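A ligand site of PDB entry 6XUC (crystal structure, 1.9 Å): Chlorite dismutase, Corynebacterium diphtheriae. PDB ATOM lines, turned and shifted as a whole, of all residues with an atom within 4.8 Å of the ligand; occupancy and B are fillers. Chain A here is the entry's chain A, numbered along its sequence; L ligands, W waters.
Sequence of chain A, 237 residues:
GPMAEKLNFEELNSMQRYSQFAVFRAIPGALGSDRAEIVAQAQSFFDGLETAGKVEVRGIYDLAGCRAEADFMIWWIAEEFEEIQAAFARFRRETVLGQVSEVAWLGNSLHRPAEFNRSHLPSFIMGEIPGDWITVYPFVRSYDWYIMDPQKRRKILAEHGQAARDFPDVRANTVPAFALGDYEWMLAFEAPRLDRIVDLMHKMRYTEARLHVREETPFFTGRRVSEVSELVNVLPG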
ATOM      1  N   ALA A 114      10.311  -9.715 -17.147  1.00  0.00           N
ATOM      2  CA  ALA A 114       9.405 -10.774 -17.525  1.00  0.00           C
ATOM      3  C   ALA A 114      10.143 -12.104 -17.494  1.00  0.00           C
ATOM      4  O   ALA A 114      11.366 -12.169 -17.474  1.00  0.00           O
ATOM      5  CB  ALA A 114       8.828 -10.519 -18.917  1.00  0.00           C
ATOM      6  N   GLU A 115       9.374 -13.178 -17.473  1.00  0.00           N
ATOM      7  CA  GLU A 115       9.959 -14.489 -17.234  1.00  0.00           C
ATOM      8  C   GLU A 115      10.791 -14.949 -18.398  1.00  0.00           C
ATOM      9  O   GLU A 115      11.886 -15.511 -18.213  1.00  0.00           O
ATOM     10  CB  GLU A 115       8.825 -15.485 -16.939  1.00  0.00           C
ATOM     11  CG  GLU A 115       9.286 -16.851 -16.580  1.00  0.00           C
ATOM     12  CD  GLU A 115       8.148 -17.766 -16.186  1.00  0.00           C
ATOM     13  OE1 GLU A 115       6.941 -17.450 -16.393  1.00  0.00           O
ATOM     14  OE2 GLU A 115       8.480 -18.816 -15.660  1.00  0.00           O
ATOM     15  N   ASN A 117      10.642 -13.107 -21.898  1.00  0.00           N
ATOM     16  CA  ASN A 117      10.901 -12.090 -22.918  1.00  0.00           C
ATOM     17  C   ASN A 117      11.281 -10.807 -22.210  1.00  0.00           C
ATOM     18  O   ASN A 117      10.429 -10.029 -21.808  1.00  0.00           O
ATOM     19  CB  ASN A 117       9.695 -11.899 -23.841  1.00  0.00           C
ATOM     20  CG  ASN A 117       9.952 -10.844 -24.904  1.00  0.00           C
ATOM     21  OD1 ASN A 117      11.015 -10.239 -24.931  1.00  0.00           O
ATOM     22  ND2 ASN A 117       8.991 -10.641 -25.769  1.00  0.00           N
ATOM     23  N   HIS A 120       9.875  -7.341 -22.944  1.00  0.00           N
ATOM     24  CA  HIS A 120       8.514  -6.988 -22.552  1.00  0.00           C
ATOM     25  C   HIS A 120       8.613  -6.204 -21.253  1.00  0.00           C
ATOM     26  O   HIS A 120       9.030  -6.741 -20.221  1.00  0.00           O
ATOM     27  CB  HIS A 120       7.683  -8.267 -22.401  1.00  0.00           C
ATOM     28  CG  HIS A 120       6.348  -8.029 -21.745  1.00  0.00           C
ATOM     29  ND1 HIS A 120       5.256  -7.545 -22.430  1.00  0.00           N
ATOM     30  CD2 HIS A 120       5.947  -8.196 -20.468  1.00  0.00           C
ATOM     31  CE1 HIS A 120       4.236  -7.414 -21.602  1.00  0.00           C
ATOM     32  NE2 HIS A 120       4.634  -7.789 -20.392  1.00  0.00           N
ATOM     33  N   TYR A 137      -6.904  -3.533 -14.058  1.00  0.00           N
ATOM     34  CA  TYR A 137      -7.534  -4.615 -13.302  1.00  0.00           C
ATOM     35  C   TYR A 137      -6.489  -5.541 -12.749  1.00  0.00           C
ATOM     36  O   TYR A 137      -5.415  -5.677 -13.328  1.00  0.00           O
ATOM     37  CB  TYR A 137      -8.529  -5.427 -14.138  1.00  0.00           C
ATOM     38  CG  TYR A 137      -8.105  -5.993 -15.450  1.00  0.00           C
ATOM     39  CD1 TYR A 137      -8.003  -5.184 -16.582  1.00  0.00           C
ATOM     40  CD2 TYR A 137      -7.922  -7.361 -15.614  1.00  0.00           C
ATOM     41  CE1 TYR A 137      -7.718  -5.736 -17.845  1.00  0.00           C
ATOM     42  CE2 TYR A 137      -7.658  -7.921 -16.879  1.00  0.00           C
ATOM     43  CZ  TYR A 137      -7.555  -7.083 -17.979  1.00  0.00           C
ATOM     44  OH  TYR A 137      -7.312  -7.635 -19.203  1.00  0.00           O
ATOM     45  N   PHE A 139      -5.063  -9.441 -11.587  1.00  0.00           N
ATOM     46  CA  PHE A 139      -5.066 -10.746 -12.239  1.00  0.00           C
ATOM     47  C   PHE A 139      -4.478 -11.805 -11.333  1.00  0.00           C
ATOM     48  O   PHE A 139      -3.503 -11.549 -10.605  1.00  0.00           O
ATOM     49  CB  PHE A 139      -4.254 -10.642 -13.539  1.00  0.00           C
ATOM     50  CG  PHE A 139      -4.635 -11.659 -14.591  1.00  0.00           C
ATOM     51  CD1 PHE A 139      -5.628 -11.382 -15.532  1.00  0.00           C
ATOM     52  CD2 PHE A 139      -3.971 -12.873 -14.661  1.00  0.00           C
ATOM     53  CE1 PHE A 139      -5.941 -12.328 -16.517  1.00  0.00           C
ATOM     54  CE2 PHE A 139      -4.258 -13.779 -15.626  1.00  0.00           C
ATOM     55  CZ  PHE A 139      -5.244 -13.524 -16.547  1.00  0.00           C
ATOM     56  N   ARG A 141      -3.483 -16.003 -11.906  1.00  0.00           N
ATOM     57  CA  ARG A 141      -3.386 -17.188 -12.746  1.00  0.00           C
ATOM     58  C   ARG A 141      -3.907 -18.467 -12.054  1.00  0.00           C
ATOM     59  O   ARG A 141      -4.029 -18.549 -10.834  1.00  0.00           O
ATOM     60  CB  ARG A 141      -1.927 -17.404 -13.151  1.00  0.00           C
ATOM     61  CG  ARG A 141      -1.444 -16.379 -14.137  1.00  0.00           C
ATOM     62  CD  ARG A 141      -1.833 -16.817 -15.548  1.00  0.00           C
ATOM     63  NE  ARG A 141      -1.427 -15.861 -16.564  1.00  0.00           N
ATOM     64  CZ  ARG A 141      -2.050 -15.710 -17.737  1.00  0.00           C
ATOM     65  NH1 ARG A 141      -3.114 -16.429 -18.045  1.00  0.00           N
ATOM     66  NH2 ARG A 141      -1.624 -14.796 -18.564  1.00  0.00           N
ATOM     67  N   TRP A 145      -0.352 -22.779 -13.302  1.00  0.00           N
ATOM     68  CA  TRP A 145       0.328 -21.986 -14.323  1.00  0.00           C
ATOM     69  C   TRP A 145       1.839 -21.983 -14.146  1.00  0.00           C
ATOM     70  O   TRP A 145       2.600 -22.175 -15.112  1.00  0.00           O
ATOM     71  CB  TRP A 145      -0.202 -20.568 -14.250  1.00  0.00           C
ATOM     72  CG  TRP A 145       0.446 -19.576 -15.164  1.00  0.00           C
ATOM     73  CD1 TRP A 145       1.188 -18.504 -14.792  1.00  0.00           C
ATOM     74  CD2 TRP A 145       0.325 -19.514 -16.606  1.00  0.00           C
ATOM     75  NE1 TRP A 145       1.556 -17.767 -15.906  1.00  0.00           N
ATOM     76  CE2 TRP A 145       1.035 -18.363 -17.028  1.00  0.00           C
ATOM     77  CE3 TRP A 145      -0.302 -20.294 -17.568  1.00  0.00           C
ATOM     78  CZ2 TRP A 145       1.149 -18.017 -18.371  1.00  0.00           C
ATOM     79  CZ3 TRP A 145      -0.225 -19.923 -18.885  1.00  0.00           C
ATOM     80  CH2 TRP A 145       0.487 -18.796 -19.275  1.00  0.00           C
ATOM     81  N   TYR A 146       2.309 -21.760 -12.906  1.00  0.00           N
ATOM     82  CA  TYR A 146       3.737 -21.536 -12.688  1.00  0.00           C
ATOM     83  C   TYR A 146       4.534 -22.835 -12.705  1.00  0.00           C
ATOM     84  O   TYR A 146       5.734 -22.823 -13.058  1.00  0.00           O
ATOM     85  CB  TYR A 146       3.958 -20.749 -11.376  1.00  0.00           C
ATOM     86  CG  TYR A 146       3.187 -19.425 -11.382  1.00  0.00           C
ATOM     87  CD1 TYR A 146       3.699 -18.290 -12.002  1.00  0.00           C
ATOM     88  CD2 TYR A 146       1.907 -19.336 -10.811  1.00  0.00           C
ATOM     89  CE1 TYR A 146       3.007 -17.083 -12.028  1.00  0.00           C
ATOM     90  CE2 TYR A 146       1.187 -18.119 -10.837  1.00  0.00           C
ATOM     91  CZ  TYR A 146       1.755 -17.009 -11.436  1.00  0.00           C
ATOM     92  OH  TYR A 146       1.075 -15.827 -11.489  1.00  0.00           O
ATOM     93  N   LEU A 157       2.759 -18.009 -23.693  1.00  0.00           N
ATOM     94  CA  LEU A 157       2.924 -16.560 -23.594  1.00  0.00           C
ATOM     95  C   LEU A 157       3.324 -15.974 -24.925  1.00  0.00           C
ATOM     96  O   LEU A 157       2.911 -14.855 -25.244  1.00  0.00           O
ATOM     97  CB  LEU A 157       3.941 -16.186 -22.517  1.00  0.00           C
ATOM     98  CG  LEU A 157       3.437 -16.394 -21.086  1.00  0.00           C
ATOM     99  CD1 LEU A 157       4.566 -16.240 -20.062  1.00  0.00           C
ATOM    100  CD2 LEU A 157       2.319 -15.423 -20.792  1.00  0.00           C
ATOM    101  N   ALA A 158       4.096 -16.692 -25.741  1.00  0.00           N
ATOM    102  CA  ALA A 158       4.434 -16.123 -27.044  1.00  0.00           C
ATOM    103  C   ALA A 158       3.194 -16.015 -27.939  1.00  0.00           C
ATOM    104  O   ALA A 158       3.030 -15.019 -28.678  1.00  0.00           O
ATOM    105  CB  ALA A 158       5.520 -16.964 -27.730  1.00  0.00           C
ATOM    106  N   HIS A 160       0.125 -15.740 -26.831  1.00  0.00           N
ATOM    107  CA  HIS A 160      -0.587 -14.639 -26.182  1.00  0.00           C
ATOM    108  C   HIS A 160      -0.058 -13.307 -26.694  1.00  0.00           C
ATOM    109  O   HIS A 160      -0.820 -12.477 -27.160  1.00  0.00           O
ATOM    110  CB  HIS A 160      -0.446 -14.833 -24.669  1.00  0.00           C
ATOM    111  CG  HIS A 160      -0.691 -13.596 -23.843  1.00  0.00           C
ATOM    112  ND1 HIS A 160      -1.883 -13.365 -23.194  1.00  0.00           N
ATOM    113  CD2 HIS A 160       0.126 -12.579 -23.491  1.00  0.00           C
ATOM    114  CE1 HIS A 160      -1.802 -12.242 -22.495  1.00  0.00           C
ATOM    115  NE2 HIS A 160      -0.605 -11.721 -22.708  1.00  0.00           N
ATOM    116  N   GLY A 161       1.264 -13.133 -26.712  1.00  0.00           N
ATOM    117  CA  GLY A 161       1.796 -11.902 -27.267  1.00  0.00           C
ATOM    118  C   GLY A 161       1.463 -11.691 -28.740  1.00  0.00           C
ATOM    119  O   GLY A 161       1.186 -10.576 -29.183  1.00  0.00           O
ATOM    120  N   ALA A 164      -1.928 -10.020 -29.707  1.00  0.00           N
ATOM    121  CA  ALA A 164      -2.050  -8.581 -29.571  1.00  0.00           C
ATOM    122  C   ALA A 164      -1.345  -7.812 -30.667  1.00  0.00           C
ATOM    123  O   ALA A 164      -1.338  -6.581 -30.614  1.00  0.00           O
ATOM    124  CB  ALA A 164      -1.482  -8.107 -28.227  1.00  0.00           C
ATOM    125  N   VAL A 170      -2.349   0.158 -28.159  1.00  0.00           N
ATOM    126  CA  VAL A 170      -2.770  -0.107 -26.785  1.00  0.00           C
ATOM    127  C   VAL A 170      -1.531  -0.583 -26.054  1.00  0.00           C
ATOM    128  O   VAL A 170      -0.960  -1.621 -26.393  1.00  0.00           O
ATOM    129  CB  VAL A 170      -3.901  -1.133 -26.729  1.00  0.00           C
ATOM    130  CG1 VAL A 170      -4.379  -1.390 -25.264  1.00  0.00           C
ATOM    131  CG2 VAL A 170      -5.056  -0.653 -27.561  1.00  0.00           C
ATOM    132  N   ALA A 172       0.666  -1.838 -22.862  1.00  0.00           N
ATOM    133  CA  ALA A 172       0.460  -2.750 -21.749  1.00  0.00           C
ATOM    134  C   ALA A 172       1.389  -2.470 -20.566  1.00  0.00           C
ATOM    135  O   ALA A 172       2.544  -2.088 -20.746  1.00  0.00           O
ATOM    136  CB  ALA A 172       0.686  -4.185 -22.234  1.00  0.00           C
ATOM    137  N   THR A 174       2.070  -4.998 -17.397  1.00  0.00           N
ATOM    138  CA  THR A 174       1.760  -6.239 -16.698  1.00  0.00           C
ATOM    139  C   THR A 174       2.773  -6.373 -15.563  1.00  0.00           C
ATOM    140  O   THR A 174       3.929  -6.698 -15.802  1.00  0.00           O
ATOM    141  CB  THR A 174       1.811  -7.410 -17.682  1.00  0.00           C
ATOM    142  OG1 THR A 174       3.156  -7.602 -18.104  1.00  0.00           O
ATOM    143  CG2 THR A 174       0.971  -7.104 -18.864  1.00  0.00           C
ATOM    144  N   TRP A 185      -0.945 -10.183 -10.271  1.00  0.00           N
ATOM    145  CA  TRP A 185      -0.508  -9.178 -11.247  1.00  0.00           C
ATOM    146  C   TRP A 185      -1.438  -7.972 -11.171  1.00  0.00           C
ATOM    147  O   TRP A 185      -2.591  -8.069 -10.770  1.00  0.00           O
ATOM    148  CB  TRP A 185      -0.454  -9.743 -12.672  1.00  0.00           C
ATOM    149  CG  TRP A 185       0.378 -10.954 -12.760  1.00  0.00           C
ATOM    150  CD1 TRP A 185      -0.014 -12.242 -12.483  1.00  0.00           C
ATOM    151  CD2 TRP A 185       1.758 -11.024 -13.113  1.00  0.00           C
ATOM    152  NE1 TRP A 185       1.050 -13.102 -12.647  1.00  0.00           N
ATOM    153  CE2 TRP A 185       2.162 -12.377 -13.003  1.00  0.00           C
ATOM    154  CE3 TRP A 185       2.715 -10.053 -13.485  1.00  0.00           C
ATOM    155  CZ2 TRP A 185       3.453 -12.793 -13.298  1.00  0.00           C
ATOM    156  CZ3 TRP A 185       3.993 -10.474 -13.786  1.00  0.00           C
ATOM    157  CH2 TRP A 185       4.361 -11.820 -13.670  1.00  0.00           C
ATOM    158  N   LEU A 187      -2.657  -5.177 -13.886  1.00  0.00           N
ATOM    159  CA  LEU A 187      -2.619  -4.903 -15.314  1.00  0.00           C
ATOM    160  C   LEU A 187      -3.207  -3.512 -15.586  1.00  0.00           C
ATOM    161  O   LEU A 187      -4.197  -3.110 -14.974  1.00  0.00           O
ATOM    162  CB  LEU A 187      -3.414  -5.934 -16.111  1.00  0.00           C
ATOM    163  CG  LEU A 187      -3.108  -7.394 -15.825  1.00  0.00           C
ATOM    164  CD1 LEU A 187      -4.031  -8.363 -16.579  1.00  0.00           C
ATOM    165  CD2 LEU A 187      -1.693  -7.706 -16.133  1.00  0.00           C
ATOM    166  N   PHE A 189      -3.907  -1.077 -19.213  1.00  0.00           N
ATOM    167  CA  PHE A 189      -3.827  -0.945 -20.666  1.00  0.00           C
ATOM    168  C   PHE A 189      -4.241   0.463 -21.035  1.00  0.00           C
ATOM    169  O   PHE A 189      -5.314   0.920 -20.661  1.00  0.00           O
ATOM    170  CB  PHE A 189      -4.697  -2.018 -21.299  1.00  0.00           C
ATOM    171  CG  PHE A 189      -4.270  -3.403 -20.903  1.00  0.00           C
ATOM    172  CD1 PHE A 189      -3.182  -3.957 -21.478  1.00  0.00           C
ATOM    173  CD2 PHE A 189      -4.903  -4.091 -19.883  1.00  0.00           C
ATOM    174  CE1 PHE A 189      -2.713  -5.170 -21.105  1.00  0.00           C
ATOM    175  CE2 PHE A 189      -4.461  -5.338 -19.498  1.00  0.00           C
ATOM    176  CZ  PHE A 189      -3.352  -5.886 -20.125  1.00  0.00           C
ATOM    177  N   LEU A 200      -9.118  -5.026 -27.966  1.00  0.00           N
ATOM    178  CA  LEU A 200      -7.967  -5.858 -27.559  1.00  0.00           C
ATOM    179  C   LEU A 200      -8.396  -6.929 -26.552  1.00  0.00           C
ATOM    180  O   LEU A 200      -7.987  -8.090 -26.634  1.00  0.00           O
ATOM    181  CB  LEU A 200      -6.860  -5.001 -26.958  1.00  0.00           C
ATOM    182  CG  LEU A 200      -5.764  -5.792 -26.233  1.00  0.00           C
ATOM    183  CD1 LEU A 200      -4.870  -6.566 -27.231  1.00  0.00           C
ATOM    184  CD2 LEU A 200      -4.962  -4.840 -25.394  1.00  0.00           C
ATOM    185  N   MET A 201      -9.201  -6.551 -25.572  1.00  0.00           N
ATOM    186  CA  MET A 201      -9.592  -7.512 -24.552  1.00  0.00           C
ATOM    187  C   MET A 201     -10.371  -8.670 -25.178  1.00  0.00           C
ATOM    188  O   MET A 201     -10.140  -9.832 -24.834  1.00  0.00           O
ATOM    189  CB  MET A 201     -10.397  -6.801 -23.471  1.00  0.00           C
ATOM    190  CG  MET A 201      -9.697  -6.612 -22.122  1.00  0.00           C
ATOM    191  SD  MET A 201      -7.973  -6.277 -22.165  1.00  0.00           S
ATOM    192  CE  MET A 201      -7.842  -4.601 -22.689  1.00  0.00           C
ATOM    193  N   MET A 204      -7.989 -10.905 -27.182  1.00  0.00           N
ATOM    194  CA  MET A 204      -7.108 -11.682 -26.311  1.00  0.00           C
ATOM    195  C   MET A 204      -7.812 -12.876 -25.651  1.00  0.00           C
ATOM    196  O   MET A 204      -7.138 -13.705 -25.060  1.00  0.00           O
ATOM    197  CB  MET A 204      -6.497 -10.724 -25.281  1.00  0.00           C
ATOM    198  CG  MET A 204      -5.503  -9.743 -25.854  1.00  0.00           C
ATOM    199  SD  MET A 204      -4.127 -10.551 -26.655  1.00  0.00           S
ATOM    200  CE  MET A 204      -3.027 -10.735 -25.240  1.00  0.00           C
ATOM    201  N   ARG A 205      -9.150 -12.978 -25.726  1.00  0.00           N
ATOM    202  CA  ARG A 205      -9.818 -14.199 -25.309  1.00  0.00           C
ATOM    203  C   ARG A 205      -9.427 -15.397 -26.166  1.00  0.00           C
ATOM    204  O   ARG A 205      -9.557 -16.552 -25.722  1.00  0.00           O
ATOM    205  CB  ARG A 205     -11.329 -14.022 -25.382  1.00  0.00           C
ATOM    206  CG  ARG A 205     -11.868 -13.015 -24.358  1.00  0.00           C
ATOM    207  CD  ARG A 205     -11.608 -13.548 -22.954  1.00  0.00           C
ATOM    208  NE  ARG A 205     -12.378 -12.937 -21.842  1.00  0.00           N
ATOM    209  CZ  ARG A 205     -12.009 -11.865 -21.135  1.00  0.00           C
ATOM    210  NH1 ARG A 205     -10.921 -11.186 -21.458  1.00  0.00           N
ATOM    211  NH2 ARG A 205     -12.747 -11.447 -20.098  1.00  0.00           N
ATOM    212  N   THR A 207      -6.925 -17.071 -26.919  1.00  0.00           N
ATOM    213  CA  THR A 207      -5.590 -17.549 -26.589  1.00  0.00           C
ATOM    214  C   THR A 207      -5.684 -18.721 -25.626  1.00  0.00           C
ATOM    215  O   THR A 207      -6.579 -18.767 -24.803  1.00  0.00           O
ATOM    216  CB  THR A 207      -4.747 -16.430 -25.967  1.00  0.00           C
ATOM    217  OG1 THR A 207      -5.437 -15.933 -24.822  1.00  0.00           O
ATOM    218  CG2 THR A 207      -4.493 -15.283 -26.999  1.00  0.00           C
ATOM    219  N   ARG A 210      -5.889 -18.348 -21.767  1.00  0.00           N
ATOM    220  CA  ARG A 210      -7.172 -18.137 -21.078  1.00  0.00           C
ATOM    221  C   ARG A 210      -7.623 -19.376 -20.319  1.00  0.00           C
ATOM    222  O   ARG A 210      -8.493 -19.256 -19.457  1.00  0.00           O
ATOM    223  CB  ARG A 210      -8.256 -17.755 -22.091  1.00  0.00           C
ATOM    224  CG  ARG A 210      -8.030 -16.385 -22.713  1.00  0.00           C
ATOM    225  CD  ARG A 210      -8.116 -15.242 -21.703  1.00  0.00           C
ATOM    226  NE  ARG A 210      -9.363 -15.254 -20.948  1.00  0.00           N
ATOM    227  CZ  ARG A 210      -9.593 -14.487 -19.899  1.00  0.00           C
ATOM    228  NH1 ARG A 210      -8.643 -13.656 -19.469  1.00  0.00           N
ATOM    229  NH2 ARG A 210     -10.747 -14.555 -19.258  1.00  0.00           N
ATOM    230  N   VAL A 213      -6.539 -19.082 -16.012  1.00  0.00           N
ATOM    231  CA  VAL A 213      -6.943 -17.865 -15.325  1.00  0.00           C
ATOM    232  C   VAL A 213      -7.906 -18.179 -14.183  1.00  0.00           C
ATOM    233  O   VAL A 213      -8.848 -18.957 -14.356  1.00  0.00           O
ATOM    234  CB  VAL A 213      -7.648 -16.878 -16.276  1.00  0.00           C
ATOM    235  CG1 VAL A 213      -8.066 -15.612 -15.518  1.00  0.00           C
ATOM    236  CG2 VAL A 213      -6.787 -16.594 -17.493  1.00  0.00           C
ATOM    237  N   GLU A 216      -9.828 -11.857 -12.447  1.00  0.00           N
ATOM    238  CA  GLU A 216      -9.394 -10.688 -13.208  1.00  0.00           C
ATOM    239  C   GLU A 216     -10.310  -9.485 -12.996  1.00  0.00           C
ATOM    240  O   GLU A 216     -10.335  -8.586 -13.814  1.00  0.00           O
ATOM    241  CB  GLU A 216      -9.256 -11.082 -14.695  1.00  0.00           C
ATOM    242  CG  GLU A 216     -10.517 -11.246 -15.411  1.00  0.00           C
ATOM    243  CD  GLU A 216     -10.351 -12.045 -16.715  1.00  0.00           C
ATOM    244  OE1 GLU A 216      -9.589 -11.605 -17.621  1.00  0.00           O
ATOM    245  OE2 GLU A 216     -11.026 -13.094 -16.833  1.00  0.00           O
HETATM  246  O1  LIG L   1       0.778 -14.307 -16.540  1.00  0.00           O
HETATM  247  C1  LIG L   1       2.041 -14.376 -16.462  1.00  0.00           C
HETATM  248  O2  LIG L   1       2.812 -15.309 -16.160  1.00  0.00           O
HETATM  249  C2  LIG L   1       2.797 -13.098 -16.809  1.00  0.00           C
HETATM  250  C3  LIG L   1       1.921 -11.860 -16.659  1.00  0.00           C
HETATM  251  C4  LIG L   1       0.922 -11.427 -17.721  1.00  0.00           C
HETATM  252  C5  LIG L   1      -0.426 -11.378 -17.664  1.00  0.00           C
HETATM  253  C6  LIG L   1      -0.909 -10.853 -18.939  1.00  0.00           C
HETATM  254  C7  LIG L   1      -2.233 -10.668 -19.387  1.00  0.00           C
HETATM  255  C8  LIG L   1      -2.657  -9.859 -20.368  1.00  0.00           C
HETATM  256  N1  LIG L   1      -1.815  -9.318 -21.310  1.00  0.00           N
HETATM  257  C9  LIG L   1      -2.588  -8.486 -22.120  1.00  0.00           C
HETATM  258  C10 LIG L   1      -2.064  -7.718 -23.171  1.00  0.00           C
HETATM  259  C11 LIG L   1      -0.842  -7.896 -23.726  1.00  0.00           C
HETATM  260  C12 LIG L   1      -0.335  -7.246 -24.909  1.00  0.00           C
HETATM  261  C13 LIG L   1       0.881  -7.751 -25.169  1.00  0.00           C
HETATM  262  C14 LIG L   1       1.192  -8.667 -24.125  1.00  0.00           C
HETATM  263  C15 LIG L   1       2.291  -9.488 -24.012  1.00  0.00           C
HETATM  264  C16 LIG L   1       2.753 -10.064 -22.890  1.00  0.00           C
HETATM  265  C17 LIG L   1       4.107 -10.476 -22.744  1.00  0.00           C
HETATM  266  C18 LIG L   1       4.234 -10.971 -21.359  1.00  0.00           C
HETATM  267  C19 LIG L   1       2.937 -10.739 -20.784  1.00  0.00           C
HETATM  268  N2  LIG L   1       2.081 -10.213 -21.725  1.00  0.00           N
HETATM  269 FE1  LIG L   1       0.078  -9.850 -21.568  1.00  0.00          FE
HETATM  270  N3  LIG L   1       0.215 -10.644 -19.745  1.00  0.00           N
HETATM  271  C20 LIG L   1       1.319 -10.955 -19.015  1.00  0.00           C
HETATM  272  C21 LIG L   1       2.590 -10.962 -19.497  1.00  0.00           C
HETATM  273  N4  LIG L   1       0.113  -8.772 -23.244  1.00  0.00           N
HETATM  274  C22 LIG L   1       5.465 -11.514 -20.634  1.00  0.00           C
HETATM  275  C23 LIG L   1       5.165 -10.440 -23.876  1.00  0.00           C
HETATM  276  C24 LIG L   1       4.939 -11.810 -24.539  1.00  0.00           C
HETATM  277  C25 LIG L   1       5.912 -12.206 -25.612  1.00  0.00           C
HETATM  278  O3  LIG L   1       6.874 -12.947 -25.300  1.00  0.00           O
HETATM  279  O4  LIG L   1       5.693 -11.830 -26.791  1.00  0.00           O
HETATM  280  C26 LIG L   1       1.820  -7.362 -26.368  1.00  0.00           C
HETATM  281  C27 LIG L   1       2.572  -6.070 -26.071  1.00  0.00           C
HETATM  282  C28 LIG L   1       3.688  -6.215 -25.034  1.00  0.00           C
HETATM  283  O5  LIG L   1       3.657  -5.425 -24.050  1.00  0.00           O
HETATM  284  O6  LIG L   1       4.625  -7.087 -25.154  1.00  0.00           O
HETATM  285  C29 LIG L   1      -1.183  -6.207 -25.702  1.00  0.00           C
HETATM  286  C30 LIG L   1      -3.959  -8.528 -21.648  1.00  0.00           C
HETATM  287  C31 LIG L   1      -4.016  -9.343 -20.580  1.00  0.00           C
HETATM  288  C32 LIG L   1      -5.195  -9.795 -19.668  1.00  0.00           C
HETATM  289  C33 LIG L   1      -6.322 -10.644 -20.305  1.00  0.00           C
HETATM  290  C34 LIG L   1      -5.914 -12.036 -20.816  1.00  0.00           C
HETATM  291  O7  LIG L   1      -5.757 -12.141 -22.068  1.00  0.00           O
HETATM  292  O8  LIG L   1      -5.820 -12.923 -19.963  1.00  0.00           O
HETATM  293  C35 LIG L   1      -5.069  -7.669 -22.281  1.00  0.00           C
HETATM  294  C36 LIG L   1      -1.243 -11.770 -16.409  1.00  0.00           C
HETATM  295  O   HOH W   1       3.006  -2.435 -24.694  1.00  0.00           O
HETATM  296  O   HOH W   2       7.133 -13.820 -22.667  1.00  0.00           O
HETATM  297  O   HOH W   3       4.444  -4.324 -21.726  1.00  0.00           O
HETATM  298  O   HOH W   4      -4.185 -14.751 -20.131  1.00  0.00           O
HETATM  299  O   HOH W   5       7.752 -13.591 -20.227  1.00  0.00           O
HETATM  300  O   HOH W   6       5.311 -15.262 -16.084  1.00  0.00           O
HETATM  301  O   HOH W   7      -8.716 -11.481 -23.043  1.00  0.00           O
HETATM  302  O   HOH W   8      -4.708 -14.262 -22.924  1.00  0.00           O
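NE2 of His 160 binds FE1 of the ligand (2.3 Å).
An oxygen (O1) of the ligand lies within salt-bridge range of the guanidinium group (NE) of Arg 141 (2.7 Å).
NE1 of Trp 145 is in hydrogen-bond range of O2 of the ligand (2.8 Å).
An oxygen (O6) of the ligand sits at hydrogen-bond distance from a ring nitrogen (ND1) of His 120, 2.8 Å away.
The guanidinium group of Arg 210 is in salt-bridge range of an oxygen (O8) of the ligand (3.0 Å).
ND2 of Asn 117 sits at hydrogen-bond distance from O3 of the ligand (3.2 Å).
Water W4 bridges O8 of the ligand (2.5 Å) and NH1 of Arg 141 (2.9 Å).
Water W6 bridges an oxygen (O2) of the ligand (2.5 Å) and the side-chain carboxylate (OE1) of Glu 115 (2.7 Å).
Water W8 lies within hydrogen-bond range of an oxygen (O7) of the ligand, the side-chain hydroxyl of Thr 207, a ring nitrogen (ND1) of His 160 and the backbone carbonyl oxygen of Met 204.
Water W3 lies within hydrogen-bond range of an oxygen (O5) of the ligand (2.7 Å), the backbone carbonyl oxygen (O) of Ala 172 (3.1 Å) and a ring nitrogen (ND1) of His 120 (3.4 Å).
Water W1 lies within hydrogen-bond range of N of Ala 172 (3.0 Å) and O5 of the ligand (3.1 Å).
Water W7 lies within hydrogen-bond range of the guanidinium group of Arg 205 (2.7 Å), the backbone carbonyl oxygen of Met 201 (2.8 Å), an oxygen (O7) of the ligand (3.2 Å) and the backbone carbonyl oxygen of Met 204 (3.4 Å).
Merely in contact with the ligand: Tyr 137 (3.1 Å), Phe 189 (3.1 Å), Ala 164 (3.2 Å), Met 201 (3.2 Å), Phe 139 (3.4 Å), Trp 185 (3.6 Å), Met 204 (3.6 Å), Leu 187 (3.6 Å), Thr 174 (3.7 Å), Ala 172 (3.7 Å), Leu 157 (3.7 Å), Ala 114 (3.9 Å) and Gly 161 (3.9 Å).
Hydrophobic or aromatic side chains that line the ligand: Ala 114, His 120, Tyr 137, Phe 139, Trp 145, His 160, Ala 164, Ala 172, Trp 185, Leu 187, Phe 189, Met 201 and Met 204.
19 residues have an atom within 4 Å of the ligand: Ala 114, Asn 117, His 120, Tyr 137, Phe 139, Arg 141, Trp 145, Leu 157, His 160, Gly 161, Ala 164, Ala 172, Thr 174, Trp 185, Leu 187, Phe 189, Met 201, Met 204 and Arg 210.
The nearest printed residue that does not touch the ligand is Leu 200 (4.01 Å).
The side-chain hydroxyl of Thr 174 lies within hydrogen-bond range of a ring nitrogen (NE2) of His 120, at 2.7 Å.
The side-chain carboxylate (OE2) of Glu 216 lies within salt-bridge range of the guanidinium group (NH2) of Arg 210 (2.8 Å).
SD of Met 201 sits at hydrogen-bond distance from OH of Tyr 137 (3.3 Å).
The backbone NH (N) of Leu 187 lies within hydrogen-bond range of the backbone carbonyl oxygen (O) of Tyr 137, at 2.9 Å.
N of Ala 164 lies within hydrogen-bond range of SD of Met 204 (3.8 Å).
The backbone carbonyl oxygen (O) of Phe 139 sits at hydrogen-bond distance from the backbone NH (N) of Trp 185 (2.9 Å).
The side-chain hydroxyl (OH) of Tyr 146 lies within hydrogen-bond range of the indole nitrogen (NE1) of Trp 185, 3.0 Å away.
The backbone carbonyl oxygen of Met 204 sits at hydrogen-bond distance from the side-chain hydroxyl of Thr 207.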
